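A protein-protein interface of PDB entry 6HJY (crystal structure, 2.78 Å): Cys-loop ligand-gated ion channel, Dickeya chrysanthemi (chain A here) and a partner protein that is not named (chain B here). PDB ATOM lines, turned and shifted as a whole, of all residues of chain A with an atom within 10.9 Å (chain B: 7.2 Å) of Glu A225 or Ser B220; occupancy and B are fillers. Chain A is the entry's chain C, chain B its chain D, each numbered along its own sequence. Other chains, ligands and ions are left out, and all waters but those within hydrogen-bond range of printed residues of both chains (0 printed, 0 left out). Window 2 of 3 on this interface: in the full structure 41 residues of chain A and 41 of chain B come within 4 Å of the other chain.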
ATOM      1  N   ALA A 213     -10.118  13.333  24.347  1.00  0.00           N
ATOM      2  CA  ALA A 213     -11.346  13.863  23.740  1.00  0.00           C
ATOM      3  C   ALA A 213     -12.149  12.805  22.972  1.00  0.00           C
ATOM      4  O   ALA A 213     -13.337  13.019  22.723  1.00  0.00           O
ATOM      5  CB  ALA A 213     -11.020  15.040  22.828  1.00  0.00           C
ATOM      6  N   SER A 214     -11.511  11.674  22.606  1.00  0.00           N
ATOM      7  CA  SER A 214     -12.147  10.569  21.879  1.00  0.00           C
ATOM      8  C   SER A 214     -13.218   9.854  22.710  1.00  0.00           C
ATOM      9  O   SER A 214     -14.184   9.349  22.137  1.00  0.00           O
ATOM     10  CB  SER A 214     -11.104   9.579  21.369  1.00  0.00           C
ATOM     11  OG  SER A 214     -10.690   8.644  22.352  1.00  0.00           O
ATOM     12  N   SER A 216     -15.138  11.395  24.898  1.00  0.00           N
ATOM     13  CA  SER A 216     -16.197  12.380  25.137  1.00  0.00           C
ATOM     14  C   SER A 216     -17.280  12.410  24.025  1.00  0.00           C
ATOM     15  O   SER A 216     -18.022  13.390  23.914  1.00  0.00           O
ATOM     16  CB  SER A 216     -15.599  13.765  25.391  1.00  0.00           C
ATOM     17  OG  SER A 216     -15.134  14.390  24.205  1.00  0.00           O
ATOM     18  N   VAL A 217     -17.384  11.324  23.228  1.00  0.00           N
ATOM     19  CA  VAL A 217     -18.401  11.172  22.177  1.00  0.00           C
ATOM     20  C   VAL A 217     -19.654  10.489  22.741  1.00  0.00           C
ATOM     21  O   VAL A 217     -20.740  10.667  22.196  1.00  0.00           O
ATOM     22  CB  VAL A 217     -17.897  10.501  20.860  1.00  0.00           C
ATOM     23  CG1 VAL A 217     -16.871  11.374  20.146  1.00  0.00           C
ATOM     24  CG2 VAL A 217     -17.357   9.088  21.088  1.00  0.00           C
ATOM     25  N   PHE A 218     -19.489   9.718  23.839  1.00  0.00           N
ATOM     26  CA  PHE A 218     -20.548   8.986  24.536  1.00  0.00           C
ATOM     27  C   PHE A 218     -21.524   9.904  25.267  1.00  0.00           C
ATOM     28  O   PHE A 218     -22.644   9.486  25.567  1.00  0.00           O
ATOM     29  CB  PHE A 218     -19.942   7.968  25.516  1.00  0.00           C
ATOM     30  CG  PHE A 218     -19.321   6.767  24.851  1.00  0.00           C
ATOM     31  CD1 PHE A 218     -20.083   5.644  24.556  1.00  0.00           C
ATOM     32  CD2 PHE A 218     -17.972   6.755  24.523  1.00  0.00           C
ATOM     33  CE1 PHE A 218     -19.505   4.531  23.938  1.00  0.00           C
ATOM     34  CE2 PHE A 218     -17.397   5.643  23.904  1.00  0.00           C
ATOM     35  CZ  PHE A 218     -18.168   4.541  23.614  1.00  0.00           C
ATOM     36  N   TRP A 219     -21.105  11.152  25.545  1.00  0.00           N
ATOM     37  CA  TRP A 219     -21.921  12.145  26.237  1.00  0.00           C
ATOM     38  C   TRP A 219     -22.863  12.899  25.282  1.00  0.00           C
ATOM     39  O   TRP A 219     -23.639  13.743  25.736  1.00  0.00           O
ATOM     40  CB  TRP A 219     -21.042  13.082  27.078  1.00  0.00           C
ATOM     41  CG  TRP A 219     -20.288  12.346  28.150  1.00  0.00           C
ATOM     42  CD1 TRP A 219     -19.001  11.903  28.088  1.00  0.00           C
ATOM     43  CD2 TRP A 219     -20.808  11.894  29.411  1.00  0.00           C
ATOM     44  NE1 TRP A 219     -18.671  11.232  29.245  1.00  0.00           N
ATOM     45  CE2 TRP A 219     -19.763  11.211  30.077  1.00  0.00           C
ATOM     46  CE3 TRP A 219     -22.053  12.016  30.054  1.00  0.00           C
ATOM     47  CZ2 TRP A 219     -19.924  10.656  31.354  1.00  0.00           C
ATOM     48  CZ3 TRP A 219     -22.212  11.466  31.317  1.00  0.00           C
ATOM     49  CH2 TRP A 219     -21.159  10.795  31.956  1.00  0.00           C
ATOM     50  N   LEU A 220     -22.829  12.558  23.971  1.00  0.00           N
ATOM     51  CA  LEU A 220     -23.723  13.118  22.953  1.00  0.00           C
ATOM     52  C   LEU A 220     -25.105  12.464  23.118  1.00  0.00           C
ATOM     53  O   LEU A 220     -25.191  11.295  23.513  1.00  0.00           O
ATOM     54  CB  LEU A 220     -23.172  12.901  21.531  1.00  0.00           C
ATOM     55  CG  LEU A 220     -22.095  13.881  21.056  1.00  0.00           C
ATOM     56  CD1 LEU A 220     -21.169  13.220  20.054  1.00  0.00           C
ATOM     57  CD2 LEU A 220     -22.720  15.132  20.445  1.00  0.00           C
ATOM     58  N   GLU A 221     -26.174  13.225  22.829  1.00  0.00           N
ATOM     59  CA  GLU A 221     -27.568  12.817  23.025  1.00  0.00           C
ATOM     60  C   GLU A 221     -28.029  11.643  22.144  1.00  0.00           C
ATOM     61  O   GLU A 221     -28.460  10.626  22.691  1.00  0.00           O
ATOM     62  CB  GLU A 221     -28.530  14.022  22.890  1.00  0.00           C
ATOM     63  CG  GLU A 221     -28.211  15.216  23.787  1.00  0.00           C
ATOM     64  CD  GLU A 221     -28.162  14.929  25.277  1.00  0.00           C
ATOM     65  OE1 GLU A 221     -29.242  14.826  25.902  1.00  0.00           O
ATOM     66  OE2 GLU A 221     -27.041  14.792  25.819  1.00  0.00           O
ATOM     67  N   SER A 222     -27.955  11.778  20.805  1.00  0.00           N
ATOM     68  CA  SER A 222     -28.409  10.733  19.879  1.00  0.00           C
ATOM     69  C   SER A 222     -27.294   9.841  19.327  1.00  0.00           C
ATOM     70  O   SER A 222     -26.119  10.209  19.377  1.00  0.00           O
ATOM     71  CB  SER A 222     -29.227  11.342  18.740  1.00  0.00           C
ATOM     72  OG  SER A 222     -28.411  11.997  17.782  1.00  0.00           O
ATOM     73  N   PHE A 223     -27.686   8.659  18.799  1.00  0.00           N
ATOM     74  CA  PHE A 223     -26.811   7.658  18.179  1.00  0.00           C
ATOM     75  C   PHE A 223     -26.188   8.213  16.892  1.00  0.00           C
ATOM     76  O   PHE A 223     -25.032   7.901  16.590  1.00  0.00           O
ATOM     77  CB  PHE A 223     -27.607   6.362  17.903  1.00  0.00           C
ATOM     78  CG  PHE A 223     -26.944   5.327  17.016  1.00  0.00           C
ATOM     79  CD1 PHE A 223     -25.918   4.524  17.502  1.00  0.00           C
ATOM     80  CD2 PHE A 223     -27.379   5.122  15.712  1.00  0.00           C
ATOM     81  CE1 PHE A 223     -25.317   3.557  16.686  1.00  0.00           C
ATOM     82  CE2 PHE A 223     -26.779   4.153  14.897  1.00  0.00           C
ATOM     83  CZ  PHE A 223     -25.754   3.376  15.392  1.00  0.00           C
ATOM     84  N   SER A 224     -26.955   9.051  16.155  1.00  0.00           N
ATOM     85  CA  SER A 224     -26.550   9.720  14.909  1.00  0.00           C
ATOM     86  C   SER A 224     -25.390  10.692  15.160  1.00  0.00           C
ATOM     87  O   SER A 224     -24.491  10.798  14.321  1.00  0.00           O
ATOM     88  CB  SER A 224     -27.734  10.457  14.290  1.00  0.00           C
ATOM     89  OG  SER A 224     -27.437  10.964  13.000  1.00  0.00           O
ATOM     90  N   GLU A 225     -25.407  11.373  16.327  1.00  0.00           N
ATOM     91  CA  GLU A 225     -24.382  12.327  16.761  1.00  0.00           C
ATOM     92  C   GLU A 225     -23.109  11.615  17.221  1.00  0.00           C
ATOM     93  O   GLU A 225     -22.022  12.007  16.797  1.00  0.00           O
ATOM     94  CB  GLU A 225     -24.921  13.248  17.876  1.00  0.00           C
ATOM     95  CG  GLU A 225     -25.917  14.289  17.385  1.00  0.00           C
ATOM     96  CD  GLU A 225     -26.800  14.889  18.467  1.00  0.00           C
ATOM     97  OE1 GLU A 225     -26.260  15.379  19.483  1.00  0.00           O
ATOM     98  OE2 GLU A 225     -28.038  14.905  18.278  1.00  0.00           O
ATOM     99  N   ARG A 226     -23.249  10.565  18.076  1.00  0.00           N
ATOM    100  CA  ARG A 226     -22.150   9.763  18.645  1.00  0.00           C
ATOM    101  C   ARG A 226     -21.292   9.101  17.566  1.00  0.00           C
ATOM    102  O   ARG A 226     -20.064   9.107  17.671  1.00  0.00           O
ATOM    103  CB  ARG A 226     -22.682   8.668  19.591  1.00  0.00           C
ATOM    104  CG  ARG A 226     -23.343   9.184  20.861  1.00  0.00           C
ATOM    105  CD  ARG A 226     -23.480   8.100  21.918  1.00  0.00           C
ATOM    106  NE  ARG A 226     -24.278   6.961  21.452  1.00  0.00           N
ATOM    107  CZ  ARG A 226     -25.602   6.868  21.544  1.00  0.00           C
ATOM    108  NH1 ARG A 226     -26.312   7.865  22.063  1.00  0.00           N
ATOM    109  NH2 ARG A 226     -26.229   5.786  21.103  1.00  0.00           N
ATOM    110  N   LEU A 227     -21.948   8.518  16.543  1.00  0.00           N
ATOM    111  CA  LEU A 227     -21.298   7.810  15.445  1.00  0.00           C
ATOM    112  C   LEU A 227     -20.544   8.744  14.499  1.00  0.00           C
ATOM    113  O   LEU A 227     -19.355   8.521  14.267  1.00  0.00           O
ATOM    114  CB  LEU A 227     -22.313   6.930  14.685  1.00  0.00           C
ATOM    115  CG  LEU A 227     -21.760   6.041  13.557  1.00  0.00           C
ATOM    116  CD1 LEU A 227     -20.787   4.984  14.090  1.00  0.00           C
ATOM    117  CD2 LEU A 227     -22.883   5.362  12.818  1.00  0.00           C
ATOM    118  N   GLN A 228     -21.223   9.791  13.974  1.00  0.00           N
ATOM    119  CA  GLN A 228     -20.643  10.771  13.045  1.00  0.00           C
ATOM    120  C   GLN A 228     -19.436  11.523  13.621  1.00  0.00           C
ATOM    121  O   GLN A 228     -18.569  11.952  12.856  1.00  0.00           O
ATOM    122  CB  GLN A 228     -21.713  11.742  12.524  1.00  0.00           C
ATOM    123  CG  GLN A 228     -22.244  11.336  11.147  1.00  0.00           C
ATOM    124  CD  GLN A 228     -23.312  12.248  10.598  1.00  0.00           C
ATOM    125  OE1 GLN A 228     -23.437  13.416  10.976  1.00  0.00           O
ATOM    126  NE2 GLN A 228     -24.077  11.734   9.649  1.00  0.00           N
ATOM    127  N   THR A 229     -19.367  11.654  14.965  1.00  0.00           N
ATOM    128  CA  THR A 229     -18.256  12.304  15.668  1.00  0.00           C
ATOM    129  C   THR A 229     -17.085  11.318  15.837  1.00  0.00           C
ATOM    130  O   THR A 229     -15.928  11.746  15.819  1.00  0.00           O
ATOM    131  CB  THR A 229     -18.734  12.971  16.974  1.00  0.00           C
ATOM    132  OG1 THR A 229     -19.929  13.706  16.714  1.00  0.00           O
ATOM    133  CG2 THR A 229     -17.702  13.931  17.556  1.00  0.00           C
ATOM    134  N   SER A 230     -17.384  10.003  15.965  1.00  0.00           N
ATOM    135  CA  SER A 230     -16.378   8.937  16.094  1.00  0.00           C
ATOM    136  C   SER A 230     -15.585   8.763  14.790  1.00  0.00           C
ATOM    137  O   SER A 230     -14.389   8.462  14.847  1.00  0.00           O
ATOM    138  CB  SER A 230     -17.027   7.624  16.511  1.00  0.00           C
ATOM    139  OG  SER A 230     -17.332   7.625  17.895  1.00  0.00           O
ATOM    140  N   PHE A 231     -16.247   8.982  13.626  1.00  0.00           N
ATOM    141  CA  PHE A 231     -15.628   8.914  12.299  1.00  0.00           C
ATOM    142  C   PHE A 231     -14.744  10.139  12.067  1.00  0.00           C
ATOM    143  O   PHE A 231     -13.759  10.052  11.330  1.00  0.00           O
ATOM    144  CB  PHE A 231     -16.683   8.802  11.182  1.00  0.00           C
ATOM    145  CG  PHE A 231     -17.314   7.442  11.023  1.00  0.00           C
ATOM    146  CD1 PHE A 231     -16.625   6.406  10.404  1.00  0.00           C
ATOM    147  CD2 PHE A 231     -18.615   7.211  11.441  1.00  0.00           C
ATOM    148  CE1 PHE A 231     -17.217   5.149  10.241  1.00  0.00           C
ATOM    149  CE2 PHE A 231     -19.213   5.961  11.259  1.00  0.00           C
ATOM    150  CZ  PHE A 231     -18.507   4.937  10.670  1.00  0.00           C
ATOM    151  N   THR A 232     -15.115  11.284  12.683  1.00  0.00           N
ATOM    152  CA  THR A 232     -14.381  12.552  12.612  1.00  0.00           C
ATOM    153  C   THR A 232     -13.062  12.406  13.386  1.00  0.00           C
ATOM    154  O   THR A 232     -12.022  12.862  12.906  1.00  0.00           O
ATOM    155  CB  THR A 232     -15.266  13.719  13.100  1.00  0.00           C
ATOM    156  OG1 THR A 232     -16.508  13.692  12.395  1.00  0.00           O
ATOM    157  CG2 THR A 232     -14.607  15.092  12.919  1.00  0.00           C
ATOM    158  N   CYS A 233     -13.109  11.735  14.560  1.00  0.00           N
ATOM    159  CA  CYS A 233     -11.952  11.440  15.414  1.00  0.00           C
ATOM    160  C   CYS A 233     -11.033  10.434  14.722  1.00  0.00           C
ATOM    161  O   CYS A 233      -9.811  10.546  14.836  1.00  0.00           O
ATOM    162  CB  CYS A 233     -12.403  10.937  16.783  1.00  0.00           C
ATOM    163  SG  CYS A 233     -13.254  12.185  17.785  1.00  0.00           S
ATOM    164  N   ALA A 271     -14.412   2.269  21.123  1.00  0.00           N
ATOM    165  CA  ALA A 271     -15.517   3.215  21.326  1.00  0.00           C
ATOM    166  C   ALA A 271     -16.650   3.016  20.315  1.00  0.00           C
ATOM    167  O   ALA A 271     -17.814   3.122  20.697  1.00  0.00           O
ATOM    168  CB  ALA A 271     -15.006   4.650  21.267  1.00  0.00           C
ATOM    169  N   ILE A 272     -16.307   2.696  19.043  1.00  0.00           N
ATOM    170  CA  ILE A 272     -17.268   2.439  17.963  1.00  0.00           C
ATOM    171  C   ILE A 272     -18.047   1.143  18.250  1.00  0.00           C
ATOM    172  O   ILE A 272     -19.273   1.141  18.114  1.00  0.00           O
ATOM    173  CB  ILE A 272     -16.600   2.500  16.550  1.00  0.00           C
ATOM    174  CG1 ILE A 272     -16.415   3.974  16.123  1.00  0.00           C
ATOM    175  CG2 ILE A 272     -17.391   1.716  15.471  1.00  0.00           C
ATOM    176  CD1 ILE A 272     -15.567   4.239  14.870  1.00  0.00           C
ATOM    177  N   ILE A 275     -20.618   1.929  21.040  1.00  0.00           N
ATOM    178  CA  ILE A 275     -21.762   2.712  20.546  1.00  0.00           C
ATOM    179  C   ILE A 275     -22.783   1.772  19.868  1.00  0.00           C
ATOM    180  O   ILE A 275     -23.982   1.889  20.131  1.00  0.00           O
ATOM    181  CB  ILE A 275     -21.323   3.924  19.649  1.00  0.00           C
ATOM    182  CG1 ILE A 275     -20.586   4.997  20.487  1.00  0.00           C
ATOM    183  CG2 ILE A 275     -22.518   4.561  18.901  1.00  0.00           C
ATOM    184  CD1 ILE A 275     -19.789   6.076  19.691  1.00  0.00           C
ATOM    185  N   HIS A 279     -27.372   0.576  20.634  1.00  0.00           N
ATOM    186  CA  HIS A 279     -28.448   0.827  19.675  1.00  0.00           C
ATOM    187  C   HIS A 279     -29.136  -0.466  19.210  1.00  0.00           C
ATOM    188  O   HIS A 279     -30.243  -0.747  19.673  1.00  0.00           O
ATOM    189  CB  HIS A 279     -27.897   1.648  18.491  1.00  0.00           C
ATOM    190  CG  HIS A 279     -28.939   2.317  17.644  1.00  0.00           C
ATOM    191  ND1 HIS A 279     -29.692   3.375  18.120  1.00  0.00           N
ATOM    192  CD2 HIS A 279     -29.264   2.096  16.350  1.00  0.00           C
ATOM    193  CE1 HIS A 279     -30.473   3.736  17.118  1.00  0.00           C
ATOM    194  NE2 HIS A 279     -30.251   3.000  16.031  1.00  0.00           N
ATOM    195  N   LEU B 216     -23.555  29.887  17.962  1.00  0.00           N
ATOM    196  CA  LEU B 216     -24.494  28.834  17.567  1.00  0.00           C
ATOM    197  C   LEU B 216     -25.604  28.650  18.603  1.00  0.00           C
ATOM    198  O   LEU B 216     -25.395  28.890  19.797  1.00  0.00           O
ATOM    199  CB  LEU B 216     -23.771  27.503  17.286  1.00  0.00           C
ATOM    200  CG  LEU B 216     -23.043  27.394  15.941  1.00  0.00           C
ATOM    201  CD1 LEU B 216     -21.966  26.334  15.997  1.00  0.00           C
ATOM    202  CD2 LEU B 216     -24.013  27.099  14.797  1.00  0.00           C
ATOM    203  N   GLU B 217     -26.787  28.229  18.128  1.00  0.00           N
ATOM    204  CA  GLU B 217     -27.994  28.065  18.934  1.00  0.00           C
ATOM    205  C   GLU B 217     -27.976  26.843  19.855  1.00  0.00           C
ATOM    206  O   GLU B 217     -28.160  27.005  21.064  1.00  0.00           O
ATOM    207  CB  GLU B 217     -29.262  28.069  18.044  1.00  0.00           C
ATOM    208  CG  GLU B 217     -29.404  29.274  17.117  1.00  0.00           C
ATOM    209  CD  GLU B 217     -29.448  30.625  17.806  1.00  0.00           C
ATOM    210  OE1 GLU B 217     -30.505  30.961  18.389  1.00  0.00           O
ATOM    211  OE2 GLU B 217     -28.420  31.341  17.783  1.00  0.00           O
ATOM    212  N   SER B 218     -27.766  25.635  19.298  1.00  0.00           N
ATOM    213  CA  SER B 218     -27.782  24.386  20.064  1.00  0.00           C
ATOM    214  C   SER B 218     -26.401  23.805  20.389  1.00  0.00           C
ATOM    215  O   SER B 218     -25.404  24.170  19.766  1.00  0.00           O
ATOM    216  CB  SER B 218     -28.654  23.339  19.370  1.00  0.00           C
ATOM    217  OG  SER B 218     -28.021  22.792  18.224  1.00  0.00           O
ATOM    218  N   PHE B 219     -26.373  22.895  21.388  1.00  0.00           N
ATOM    219  CA  PHE B 219     -25.200  22.171  21.886  1.00  0.00           C
ATOM    220  C   PHE B 219     -24.639  21.222  20.820  1.00  0.00           C
ATOM    221  O   PHE B 219     -23.415  21.079  20.717  1.00  0.00           O
ATOM    222  CB  PHE B 219     -25.577  21.396  23.169  1.00  0.00           C
ATOM    223  CG  PHE B 219     -24.530  20.451  23.721  1.00  0.00           C
ATOM    224  CD1 PHE B 219     -23.471  20.930  24.481  1.00  0.00           C
ATOM    225  CD2 PHE B 219     -24.631  19.080  23.518  1.00  0.00           C
ATOM    226  CE1 PHE B 219     -22.503  20.055  24.993  1.00  0.00           C
ATOM    227  CE2 PHE B 219     -23.665  18.207  24.036  1.00  0.00           C
ATOM    228  CZ  PHE B 219     -22.611  18.701  24.772  1.00  0.00           C
ATOM    229  N   SER B 220     -25.537  20.576  20.036  1.00  0.00           N
ATOM    230  CA  SER B 220     -25.209  19.645  18.943  1.00  0.00           C
ATOM    231  C   SER B 220     -24.408  20.355  17.845  1.00  0.00           C
ATOM    232  O   SER B 220     -23.481  19.768  17.284  1.00  0.00           O
ATOM    233  CB  SER B 220     -26.479  19.028  18.364  1.00  0.00           C
ATOM    234  OG  SER B 220     -26.204  17.999  17.427  1.00  0.00           O
ATOM    235  N   GLU B 221     -24.754  21.635  17.584  1.00  0.00           N
ATOM    236  CA  GLU B 221     -24.106  22.505  16.603  1.00  0.00           C
ATOM    237  C   GLU B 221     -22.737  22.976  17.104  1.00  0.00           C
ATOM    238  O   GLU B 221     -21.766  22.881  16.356  1.00  0.00           O
ATOM    239  CB  GLU B 221     -25.003  23.713  16.271  1.00  0.00           C
ATOM    240  CG  GLU B 221     -26.215  23.365  15.421  1.00  0.00           C
ATOM    241  CD  GLU B 221     -27.339  24.387  15.462  1.00  0.00           C
ATOM    242  OE1 GLU B 221     -27.075  25.584  15.204  1.00  0.00           O
ATOM    243  OE2 GLU B 221     -28.497  23.982  15.713  1.00  0.00           O
ATOM    244  N   ARG B 222     -22.668  23.477  18.366  1.00  0.00           N
ATOM    245  CA  ARG B 222     -21.459  23.997  19.030  1.00  0.00           C
ATOM    246  C   ARG B 222     -20.322  22.982  19.115  1.00  0.00           C
ATOM    247  O   ARG B 222     -19.164  23.346  18.910  1.00  0.00           O
ATOM    248  CB  ARG B 222     -21.781  24.514  20.443  1.00  0.00           C
ATOM    249  CG  ARG B 222     -22.545  25.824  20.468  1.00  0.00           C
ATOM    250  CD  ARG B 222     -22.519  26.411  21.866  1.00  0.00           C
ATOM    251  NE  ARG B 222     -23.750  27.146  22.162  1.00  0.00           N
ATOM    252  CZ  ARG B 222     -24.777  26.655  22.850  1.00  0.00           C
ATOM    253  NH1 ARG B 222     -24.740  25.413  23.321  1.00  0.00           N
ATOM    254  NH2 ARG B 222     -25.849  27.403  23.078  1.00  0.00           N
ATOM    255  N   LEU B 223     -20.648  21.720  19.443  1.00  0.00           N
ATOM    256  CA  LEU B 223     -19.673  20.643  19.600  1.00  0.00           C
ATOM    257  C   LEU B 223     -19.130  20.145  18.251  1.00  0.00           C
ATOM    258  O   LEU B 223     -17.911  20.108  18.081  1.00  0.00           O
ATOM    259  CB  LEU B 223     -20.283  19.506  20.441  1.00  0.00           C
ATOM    260  CG  LEU B 223     -19.400  18.307  20.798  1.00  0.00           C
ATOM    261  CD1 LEU B 223     -19.652  17.874  22.230  1.00  0.00           C
ATOM    262  CD2 LEU B 223     -19.711  17.123  19.895  1.00  0.00           C
ATOM    263  N   GLN B 224     -20.025  19.783  17.297  1.00  0.00           N
ATOM    264  CA  GLN B 224     -19.658  19.276  15.965  1.00  0.00           C
ATOM    265  C   GLN B 224     -18.801  20.254  15.147  1.00  0.00           C
ATOM    266  O   GLN B 224     -17.993  19.816  14.324  1.00  0.00           O
ATOM    267  CB  GLN B 224     -20.900  18.827  15.173  1.00  0.00           C
ATOM    268  CG  GLN B 224     -21.116  17.308  15.221  1.00  0.00           C
ATOM    269  CD  GLN B 224     -22.344  16.821  14.485  1.00  0.00           C
ATOM    270  OE1 GLN B 224     -22.866  17.470  13.574  1.00  0.00           O
ATOM    271  NE2 GLN B 224     -22.797  15.631  14.842  1.00  0.00           N
ATOM    272  N   THR B 225     -18.961  21.570  15.395  1.00  0.00           N
ATOM    273  CA  THR B 225     -18.190  22.625  14.730  1.00  0.00           C
ATOM    274  C   THR B 225     -16.809  22.774  15.393  1.00  0.00           C
ATOM    275  O   THR B 225     -15.842  23.113  14.708  1.00  0.00           O
ATOM    276  CB  THR B 225     -19.007  23.929  14.639  1.00  0.00           C
ATOM    277  OG1 THR B 225     -20.327  23.629  14.187  1.00  0.00           O
ATOM    278  CG2 THR B 225     -18.391  24.943  13.684  1.00  0.00           C
ATOM    279  N   ILE B 271     -17.993  24.415  26.593  1.00  0.00           N
ATOM    280  CA  ILE B 271     -19.255  23.897  26.055  1.00  0.00           C
ATOM    281  C   ILE B 271     -19.771  22.740  26.938  1.00  0.00           C
ATOM    282  O   ILE B 271     -20.968  22.701  27.234  1.00  0.00           O
ATOM    283  CB  ILE B 271     -19.153  23.551  24.530  1.00  0.00           C
ATOM    284  CG1 ILE B 271     -18.806  24.811  23.698  1.00  0.00           C
ATOM    285  CG2 ILE B 271     -20.442  22.909  23.993  1.00  0.00           C
ATOM    286  CD1 ILE B 271     -18.123  24.548  22.332  1.00  0.00           C
ATOM    287  N   HIS B 275     -23.767  21.952  29.571  1.00  0.00           N
ATOM    288  CA  HIS B 275     -24.708  20.847  29.380  1.00  0.00           C
ATOM    289  C   HIS B 275     -24.852  19.978  30.638  1.00  0.00           C
ATOM    290  O   HIS B 275     -25.843  20.132  31.351  1.00  0.00           O
ATOM    291  CB  HIS B 275     -24.300  20.021  28.144  1.00  0.00           C
ATOM    292  CG  HIS B 275     -25.386  19.150  27.586  1.00  0.00           C
ATOM    293  ND1 HIS B 275     -26.486  19.684  26.939  1.00  0.00           N
ATOM    294  CD2 HIS B 275     -25.467  17.800  27.546  1.00  0.00           C
ATOM    295  CE1 HIS B 275     -27.215  18.651  26.561  1.00  0.00           C
ATOM    296  NE2 HIS B 275     -26.645  17.495  26.900  1.00  0.00           N
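The side-chain carboxylate (OE2) of Glu A221 is in hydrogen-bond range of a ring nitrogen (NE2) of His B275, 2.9 Å away.
The side-chain hydroxyl (OG) of Ser B220 sits at hydrogen-bond distance from the side-chain carboxylate (OE1) of Glu A225, 3.3 Å away.
The side-chain carboxylate of Glu A225 is in hydrogen-bond range of the side-chain hydroxyl of Ser A222 (3.0 Å).
The side-chain hydroxyl (OG1) of Thr A229 sits at hydrogen-bond distance from the backbone carbonyl oxygen (O) of Glu A225, 2.7 Å away.
The backbone carbonyl oxygen (O) of Thr A229 lies within hydrogen-bond range of the side-chain sulfur (SG) of Cys A233 (3.3 Å).
Among the printed residues, merely in contact across the chains: Leu A220 with Leu B223 (3.6 Å) and Thr A229 with Gln B224 (3.9 Å).
Printed residues of chain B within 4 Å of Leu A220: Leu B223.
Printed residues of chain B within 4 Å of Glu A221: His B275.
Of chain B, only Ser B220 (3.3 Å) comes within 4 Å of Glu A225.
Ile A272 touches none of the printed residues of chain B.
No residue of chain A comes within 4 Å of Ser B218.
Ser B220 touches just one residue of chain A: Glu A225.
No residue of chain A comes within 4 Å of Glu B221.
Leu B223 touches just one residue of chain A: Leu A220.
Gln B224 touches just one residue of chain A: Thr A229.
Ile B271 touches none of the printed residues of chain A.
Printed residues of chain A within 4 Å of His B275: Glu A221 (2.9 Å).
The nearest residue of chain B that does not touch Glu A225 is Gln B224 (4.1 Å).
The nearest printed residue of chain B that does not touch Glu A221 is Phe B219 (5.1 Å).
Of the 12 printed residues of chain B, 4 touch a printed residue of chain A.
Hydrophobic or aromatic side chains of chain B within 4 Å of the printed part of chain A: Leu B223 and His B275.
Along chain B the printed residues that touch a printed residue of chain A span positions 220 to 275.
Hydrophobic or aromatic side chains of chain A that line the printed part of chain B: Leu A220.
Along chain A the printed residues that touch a printed residue of chain B span positions 220 to 229.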
